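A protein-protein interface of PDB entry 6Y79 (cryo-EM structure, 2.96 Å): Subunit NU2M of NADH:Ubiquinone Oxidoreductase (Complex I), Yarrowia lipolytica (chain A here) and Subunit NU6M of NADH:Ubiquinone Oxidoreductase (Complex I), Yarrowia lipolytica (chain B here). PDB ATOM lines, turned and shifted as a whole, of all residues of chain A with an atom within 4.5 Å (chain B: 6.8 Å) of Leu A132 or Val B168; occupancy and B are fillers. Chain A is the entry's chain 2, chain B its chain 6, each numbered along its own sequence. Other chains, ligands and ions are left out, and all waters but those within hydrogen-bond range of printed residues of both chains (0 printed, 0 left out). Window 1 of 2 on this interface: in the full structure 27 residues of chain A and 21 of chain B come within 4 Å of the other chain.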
ATOM      1  N   ILE A 109       5.681  21.290  -9.338  1.00  0.00           N
ATOM      2  CA  ILE A 109       6.803  21.140 -10.263  1.00  0.00           C
ATOM      3  C   ILE A 109       7.661  19.936  -9.879  1.00  0.00           C
ATOM      4  O   ILE A 109       8.159  19.209 -10.750  1.00  0.00           O
ATOM      5  CB  ILE A 109       7.607  22.456 -10.319  1.00  0.00           C
ATOM      6  CG1 ILE A 109       6.774  23.554 -10.967  1.00  0.00           C
ATOM      7  CG2 ILE A 109       8.865  22.317 -11.128  1.00  0.00           C
ATOM      8  CD1 ILE A 109       7.392  24.914 -10.875  1.00  0.00           C
ATOM      9  N   LEU A 112       5.779  16.847 -10.977  1.00  0.00           N
ATOM     10  CA  LEU A 112       5.985  16.729 -12.418  1.00  0.00           C
ATOM     11  C   LEU A 112       7.324  16.083 -12.745  1.00  0.00           C
ATOM     12  O   LEU A 112       7.393  15.142 -13.544  1.00  0.00           O
ATOM     13  CB  LEU A 112       5.908  18.108 -13.056  1.00  0.00           C
ATOM     14  CG  LEU A 112       6.205  18.138 -14.539  1.00  0.00           C
ATOM     15  CD1 LEU A 112       5.103  17.432 -15.243  1.00  0.00           C
ATOM     16  CD2 LEU A 112       6.290  19.540 -14.994  1.00  0.00           C
ATOM     17  N   GLY A 113       8.401  16.587 -12.143  1.00  0.00           N
ATOM     18  CA  GLY A 113       9.714  16.022 -12.395  1.00  0.00           C
ATOM     19  C   GLY A 113       9.881  14.619 -11.861  1.00  0.00           C
ATOM     20  O   GLY A 113      10.682  13.848 -12.386  1.00  0.00           O
ATOM     21  N   VAL A 128      16.635  15.439 -17.870  1.00  0.00           N
ATOM     22  CA  VAL A 128      15.879  16.680 -17.703  1.00  0.00           C
ATOM     23  C   VAL A 128      14.911  16.573 -16.536  1.00  0.00           C
ATOM     24  O   VAL A 128      14.793  17.503 -15.728  1.00  0.00           O
ATOM     25  CB  VAL A 128      15.153  17.036 -19.012  1.00  0.00           C
ATOM     26  CG1 VAL A 128      14.228  18.211 -18.835  1.00  0.00           C
ATOM     27  CG2 VAL A 128      16.139  17.391 -20.059  1.00  0.00           C
ATOM     28  N   ALA A 129      14.302  15.397 -16.353  1.00  0.00           N
ATOM     29  CA  ALA A 129      13.409  15.200 -15.221  1.00  0.00           C
ATOM     30  C   ALA A 129      14.151  15.106 -13.892  1.00  0.00           C
ATOM     31  O   ALA A 129      13.640  15.586 -12.870  1.00  0.00           O
ATOM     32  CB  ALA A 129      12.585  13.955 -15.456  1.00  0.00           C
ATOM     33  N   ILE A 130      15.354  14.517 -13.884  1.00  0.00           N
ATOM     34  CA  ILE A 130      16.155  14.451 -12.664  1.00  0.00           C
ATOM     35  C   ILE A 130      16.551  15.844 -12.211  1.00  0.00           C
ATOM     36  O   ILE A 130      16.497  16.164 -11.020  1.00  0.00           O
ATOM     37  CB  ILE A 130      17.382  13.546 -12.885  1.00  0.00           C
ATOM     38  CG1 ILE A 130      17.015  12.100 -12.666  1.00  0.00           C
ATOM     39  CG2 ILE A 130      18.504  13.833 -11.924  1.00  0.00           C
ATOM     40  CD1 ILE A 130      18.033  11.198 -13.216  1.00  0.00           C
ATOM     41  N   GLU A 131      16.885  16.716 -13.153  1.00  0.00           N
ATOM     42  CA  GLU A 131      17.287  18.059 -12.751  1.00  0.00           C
ATOM     43  C   GLU A 131      16.093  18.929 -12.403  1.00  0.00           C
ATOM     44  O   GLU A 131      16.199  19.792 -11.531  1.00  0.00           O
ATOM     45  CB  GLU A 131      18.160  18.714 -13.814  1.00  0.00           C
ATOM     46  CG  GLU A 131      19.581  18.551 -13.410  1.00  0.00           C
ATOM     47  CD  GLU A 131      20.005  17.113 -13.523  1.00  0.00           C
ATOM     48  OE1 GLU A 131      19.902  16.578 -14.634  1.00  0.00           O
ATOM     49  OE2 GLU A 131      20.282  16.527 -12.466  1.00  0.00           O
ATOM     50  N   LEU A 132      14.944  18.696 -13.041  1.00  0.00           N
ATOM     51  CA  LEU A 132      13.709  19.368 -12.644  1.00  0.00           C
ATOM     52  C   LEU A 132      13.350  19.059 -11.194  1.00  0.00           C
ATOM     53  O   LEU A 132      13.133  19.973 -10.381  1.00  0.00           O
ATOM     54  CB  LEU A 132      12.589  18.941 -13.584  1.00  0.00           C
ATOM     55  CG  LEU A 132      11.204  19.553 -13.493  1.00  0.00           C
ATOM     56  CD1 LEU A 132      11.299  21.037 -13.625  1.00  0.00           C
ATOM     57  CD2 LEU A 132      10.382  19.006 -14.614  1.00  0.00           C
ATOM     58  N   GLN A 133      13.374  17.776 -10.829  1.00  0.00           N
ATOM     59  CA  GLN A 133      13.066  17.430  -9.448  1.00  0.00           C
ATOM     60  C   GLN A 133      14.195  17.805  -8.491  1.00  0.00           C
ATOM     61  O   GLN A 133      13.928  18.122  -7.329  1.00  0.00           O
ATOM     62  CB  GLN A 133      12.716  15.950  -9.336  1.00  0.00           C
ATOM     63  CG  GLN A 133      13.834  15.000  -9.544  1.00  0.00           C
ATOM     64  CD  GLN A 133      13.662  13.748  -8.726  1.00  0.00           C
ATOM     65  OE1 GLN A 133      12.604  13.506  -8.155  1.00  0.00           O
ATOM     66  NE2 GLN A 133      14.708  12.939  -8.665  1.00  0.00           N
ATOM     67  N   SER A 134      15.443  17.864  -8.960  1.00  0.00           N
ATOM     68  CA  SER A 134      16.535  18.243  -8.070  1.00  0.00           C
ATOM     69  C   SER A 134      16.506  19.726  -7.739  1.00  0.00           C
ATOM     70  O   SER A 134      16.682  20.099  -6.577  1.00  0.00           O
ATOM     71  CB  SER A 134      17.873  17.861  -8.682  1.00  0.00           C
ATOM     72  OG  SER A 134      18.058  16.465  -8.620  1.00  0.00           O
ATOM     73  N   TYR A 135      16.270  20.584  -8.738  1.00  0.00           N
ATOM     74  CA  TYR A 135      16.132  22.012  -8.467  1.00  0.00           C
ATOM     75  C   TYR A 135      14.915  22.285  -7.608  1.00  0.00           C
ATOM     76  O   TYR A 135      14.934  23.187  -6.761  1.00  0.00           O
ATOM     77  CB  TYR A 135      16.012  22.834  -9.748  1.00  0.00           C
ATOM     78  CG  TYR A 135      17.012  22.611 -10.852  1.00  0.00           C
ATOM     79  CD1 TYR A 135      18.294  22.152 -10.602  1.00  0.00           C
ATOM     80  CD2 TYR A 135      16.655  22.878 -12.165  1.00  0.00           C
ATOM     81  CE1 TYR A 135      19.180  21.950 -11.627  1.00  0.00           C
ATOM     82  CE2 TYR A 135      17.532  22.681 -13.191  1.00  0.00           C
ATOM     83  CZ  TYR A 135      18.792  22.220 -12.918  1.00  0.00           C
ATOM     84  OH  TYR A 135      19.671  22.026 -13.945  1.00  0.00           O
ATOM     85  N   SER A 136      13.851  21.501  -7.791  1.00  0.00           N
ATOM     86  CA  SER A 136      12.694  21.664  -6.926  1.00  0.00           C
ATOM     87  C   SER A 136      12.992  21.266  -5.482  1.00  0.00           C
ATOM     88  O   SER A 136      12.489  21.906  -4.560  1.00  0.00           O
ATOM     89  CB  SER A 136      11.527  20.873  -7.485  1.00  0.00           C
ATOM     90  OG  SER A 136      11.183  21.366  -8.759  1.00  0.00           O
ATOM     91  N   LEU B 163       9.409  21.311 -24.274  1.00  0.00           N
ATOM     92  CA  LEU B 163       8.372  21.869 -23.408  1.00  0.00           C
ATOM     93  C   LEU B 163       8.629  21.589 -21.921  1.00  0.00           C
ATOM     94  O   LEU B 163       8.351  22.438 -21.060  1.00  0.00           O
ATOM     95  CB  LEU B 163       7.008  21.346 -23.843  1.00  0.00           C
ATOM     96  CG  LEU B 163       6.545  21.711 -25.259  1.00  0.00           C
ATOM     97  CD1 LEU B 163       5.064  21.545 -25.370  1.00  0.00           C
ATOM     98  CD2 LEU B 163       6.911  23.126 -25.634  1.00  0.00           C
ATOM     99  N   VAL B 164       9.182  20.420 -21.591  1.00  0.00           N
ATOM    100  CA  VAL B 164       9.634  20.175 -20.220  1.00  0.00           C
ATOM    101  C   VAL B 164      10.801  21.095 -19.878  1.00  0.00           C
ATOM    102  O   VAL B 164      10.929  21.572 -18.741  1.00  0.00           O
ATOM    103  CB  VAL B 164       9.974  18.679 -20.053  1.00  0.00           C
ATOM    104  CG1 VAL B 164      10.547  18.382 -18.696  1.00  0.00           C
ATOM    105  CG2 VAL B 164       8.730  17.871 -20.230  1.00  0.00           C
ATOM    106  N   LEU B 165      11.611  21.435 -20.877  1.00  0.00           N
ATOM    107  CA  LEU B 165      12.675  22.413 -20.703  1.00  0.00           C
ATOM    108  C   LEU B 165      12.116  23.808 -20.452  1.00  0.00           C
ATOM    109  O   LEU B 165      12.718  24.601 -19.722  1.00  0.00           O
ATOM    110  CB  LEU B 165      13.550  22.389 -21.946  1.00  0.00           C
ATOM    111  CG  LEU B 165      14.928  23.002 -21.939  1.00  0.00           C
ATOM    112  CD1 LEU B 165      15.793  22.255 -20.957  1.00  0.00           C
ATOM    113  CD2 LEU B 165      15.469  22.876 -23.338  1.00  0.00           C
ATOM    114  N   ALA B 166      10.965  24.122 -21.052  1.00  0.00           N
ATOM    115  CA  ALA B 166      10.268  25.367 -20.726  1.00  0.00           C
ATOM    116  C   ALA B 166       9.811  25.386 -19.280  1.00  0.00           C
ATOM    117  O   ALA B 166       9.835  26.435 -18.631  1.00  0.00           O
ATOM    118  CB  ALA B 166       9.061  25.560 -21.630  1.00  0.00           C
ATOM    119  N   ILE B 167       9.366  24.238 -18.767  1.00  0.00           N
ATOM    120  CA  ILE B 167       9.026  24.158 -17.345  1.00  0.00           C
ATOM    121  C   ILE B 167      10.267  24.365 -16.472  1.00  0.00           C
ATOM    122  O   ILE B 167      10.198  24.989 -15.408  1.00  0.00           O
ATOM    123  CB  ILE B 167       8.322  22.827 -17.034  1.00  0.00           C
ATOM    124  CG1 ILE B 167       7.108  22.645 -17.940  1.00  0.00           C
ATOM    125  CG2 ILE B 167       7.871  22.788 -15.596  1.00  0.00           C
ATOM    126  CD1 ILE B 167       6.028  23.664 -17.725  1.00  0.00           C
ATOM    127  N   VAL B 168      11.426  23.882 -16.925  1.00  0.00           N
ATOM    128  CA  VAL B 168      12.666  24.086 -16.165  1.00  0.00           C
ATOM    129  C   VAL B 168      13.072  25.562 -16.153  1.00  0.00           C
ATOM    130  O   VAL B 168      13.499  26.098 -15.123  1.00  0.00           O
ATOM    131  CB  VAL B 168      13.792  23.196 -16.723  1.00  0.00           C
ATOM    132  CG1 VAL B 168      15.067  23.426 -15.968  1.00  0.00           C
ATOM    133  CG2 VAL B 168      13.420  21.744 -16.625  1.00  0.00           C
ATOM    134  N   LEU B 169      12.928  26.243 -17.291  1.00  0.00           N
ATOM    135  CA  LEU B 169      13.205  27.679 -17.348  1.00  0.00           C
ATOM    136  C   LEU B 169      12.222  28.470 -16.495  1.00  0.00           C
ATOM    137  O   LEU B 169      12.600  29.456 -15.846  1.00  0.00           O
ATOM    138  CB  LEU B 169      13.136  28.159 -18.789  1.00  0.00           C
ATOM    139  CG  LEU B 169      14.388  28.329 -19.625  1.00  0.00           C
ATOM    140  CD1 LEU B 169      14.911  27.008 -19.931  1.00  0.00           C
ATOM    141  CD2 LEU B 169      13.999  28.989 -20.903  1.00  0.00           C
ATOM    142  N   LEU B 170      10.955  28.047 -16.494  1.00  0.00           N
ATOM    143  CA  LEU B 170       9.943  28.619 -15.612  1.00  0.00           C
ATOM    144  C   LEU B 170      10.344  28.480 -14.154  1.00  0.00           C
ATOM    145  O   LEU B 170      10.212  29.424 -13.379  1.00  0.00           O
ATOM    146  CB  LEU B 170       8.605  27.930 -15.872  1.00  0.00           C
ATOM    147  CG  LEU B 170       7.279  28.389 -15.277  1.00  0.00           C
ATOM    148  CD1 LEU B 170       6.209  28.106 -16.283  1.00  0.00           C
ATOM    149  CD2 LEU B 170       6.966  27.645 -13.997  1.00  0.00           C
ATOM    150  N   LEU B 171      10.843  27.305 -13.773  1.00  0.00           N
ATOM    151  CA  LEU B 171      11.310  27.077 -12.408  1.00  0.00           C
ATOM    152  C   LEU B 171      12.504  27.957 -12.068  1.00  0.00           C
ATOM    153  O   LEU B 171      12.602  28.481 -10.954  1.00  0.00           O
ATOM    154  CB  LEU B 171      11.669  25.608 -12.239  1.00  0.00           C
ATOM    155  CG  LEU B 171      12.266  25.137 -10.927  1.00  0.00           C
ATOM    156  CD1 LEU B 171      11.233  25.228  -9.851  1.00  0.00           C
ATOM    157  CD2 LEU B 171      12.718  23.725 -11.114  1.00  0.00           C
ATOM    158  N   GLY B 172      13.411  28.148 -13.027  1.00  0.00           N
ATOM    159  CA  GLY B 172      14.517  29.075 -12.844  1.00  0.00           C
ATOM    160  C   GLY B 172      14.098  30.527 -12.737  1.00  0.00           C
ATOM    161  O   GLY B 172      14.871  31.349 -12.243  1.00  0.00           O
ATOM    162  N   ILE B 173      12.908  30.867 -13.226  1.00  0.00           N
ATOM    163  CA  ILE B 173      12.340  32.179 -12.928  1.00  0.00           C
ATOM    164  C   ILE B 173      11.720  32.200 -11.533  1.00  0.00           C
ATOM    165  O   ILE B 173      12.040  33.074 -10.723  1.00  0.00           O
ATOM    166  CB  ILE B 173      11.311  32.593 -13.995  1.00  0.00           C
ATOM    167  CG1 ILE B 173      11.985  32.831 -15.339  1.00  0.00           C
ATOM    168  CG2 ILE B 173      10.599  33.853 -13.580  1.00  0.00           C
ATOM    169  CD1 ILE B 173      11.016  32.944 -16.480  1.00  0.00           C
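O of Leu A132 sits at hydrogen-bond distance from OG of Ser A136 (2.9 Å).
Among the printed residues, pairs that only touch across the chains: Ile A109 with Leu B171 (3.96 Å), Leu A112 with Ile B167 (3.7 Å), Val A128 with Val B164 (3.7 Å), Leu A132 with Val B168 (3.7 Å), Leu A132 with Leu B171 (3.8 Å), Tyr A135 with Val B168 (3.8 Å), Tyr A135 with Leu B171 (3.7 Å) and Ser A136 with Leu B171 (3.7 Å).
Leu A132 touches just these residues of chain B: Val B168 (3.7 Å) and Leu B171 (3.8 Å). Of the printed residues of chain B, Tyr A135 touches Val B168 and Leu B171. Of the printed residues of chain B, Ser A136 touches Leu B171. Leu B165 touches none of the printed residues of chain A. Of the printed residues of chain A, Ile B167 touches Leu A112. Of the printed residues of chain A, Val B168 touches Leu A132 and Tyr A135. Leu B169 touches none of the printed residues of chain A. Of the printed residues of chain A, Leu B171 touches Ile A109, Leu A132, Tyr A135 and Ser A136.
Printed residues of chain B that touch a printed residue of chain A: Val B164, Ile B167, Val B168 and Leu B171. Hydrophobic or aromatic side chains of chain A that line the printed part of chain B: Ile A109, Leu A112, Val A128, Leu A132 and Tyr A135. Among the printed residues, 8 pairs touch across the chains. Among the printed residues, no Asp or Glu carboxylate lies within 4 Å of a Lys or Arg side-chain nitrogen of the other chain.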
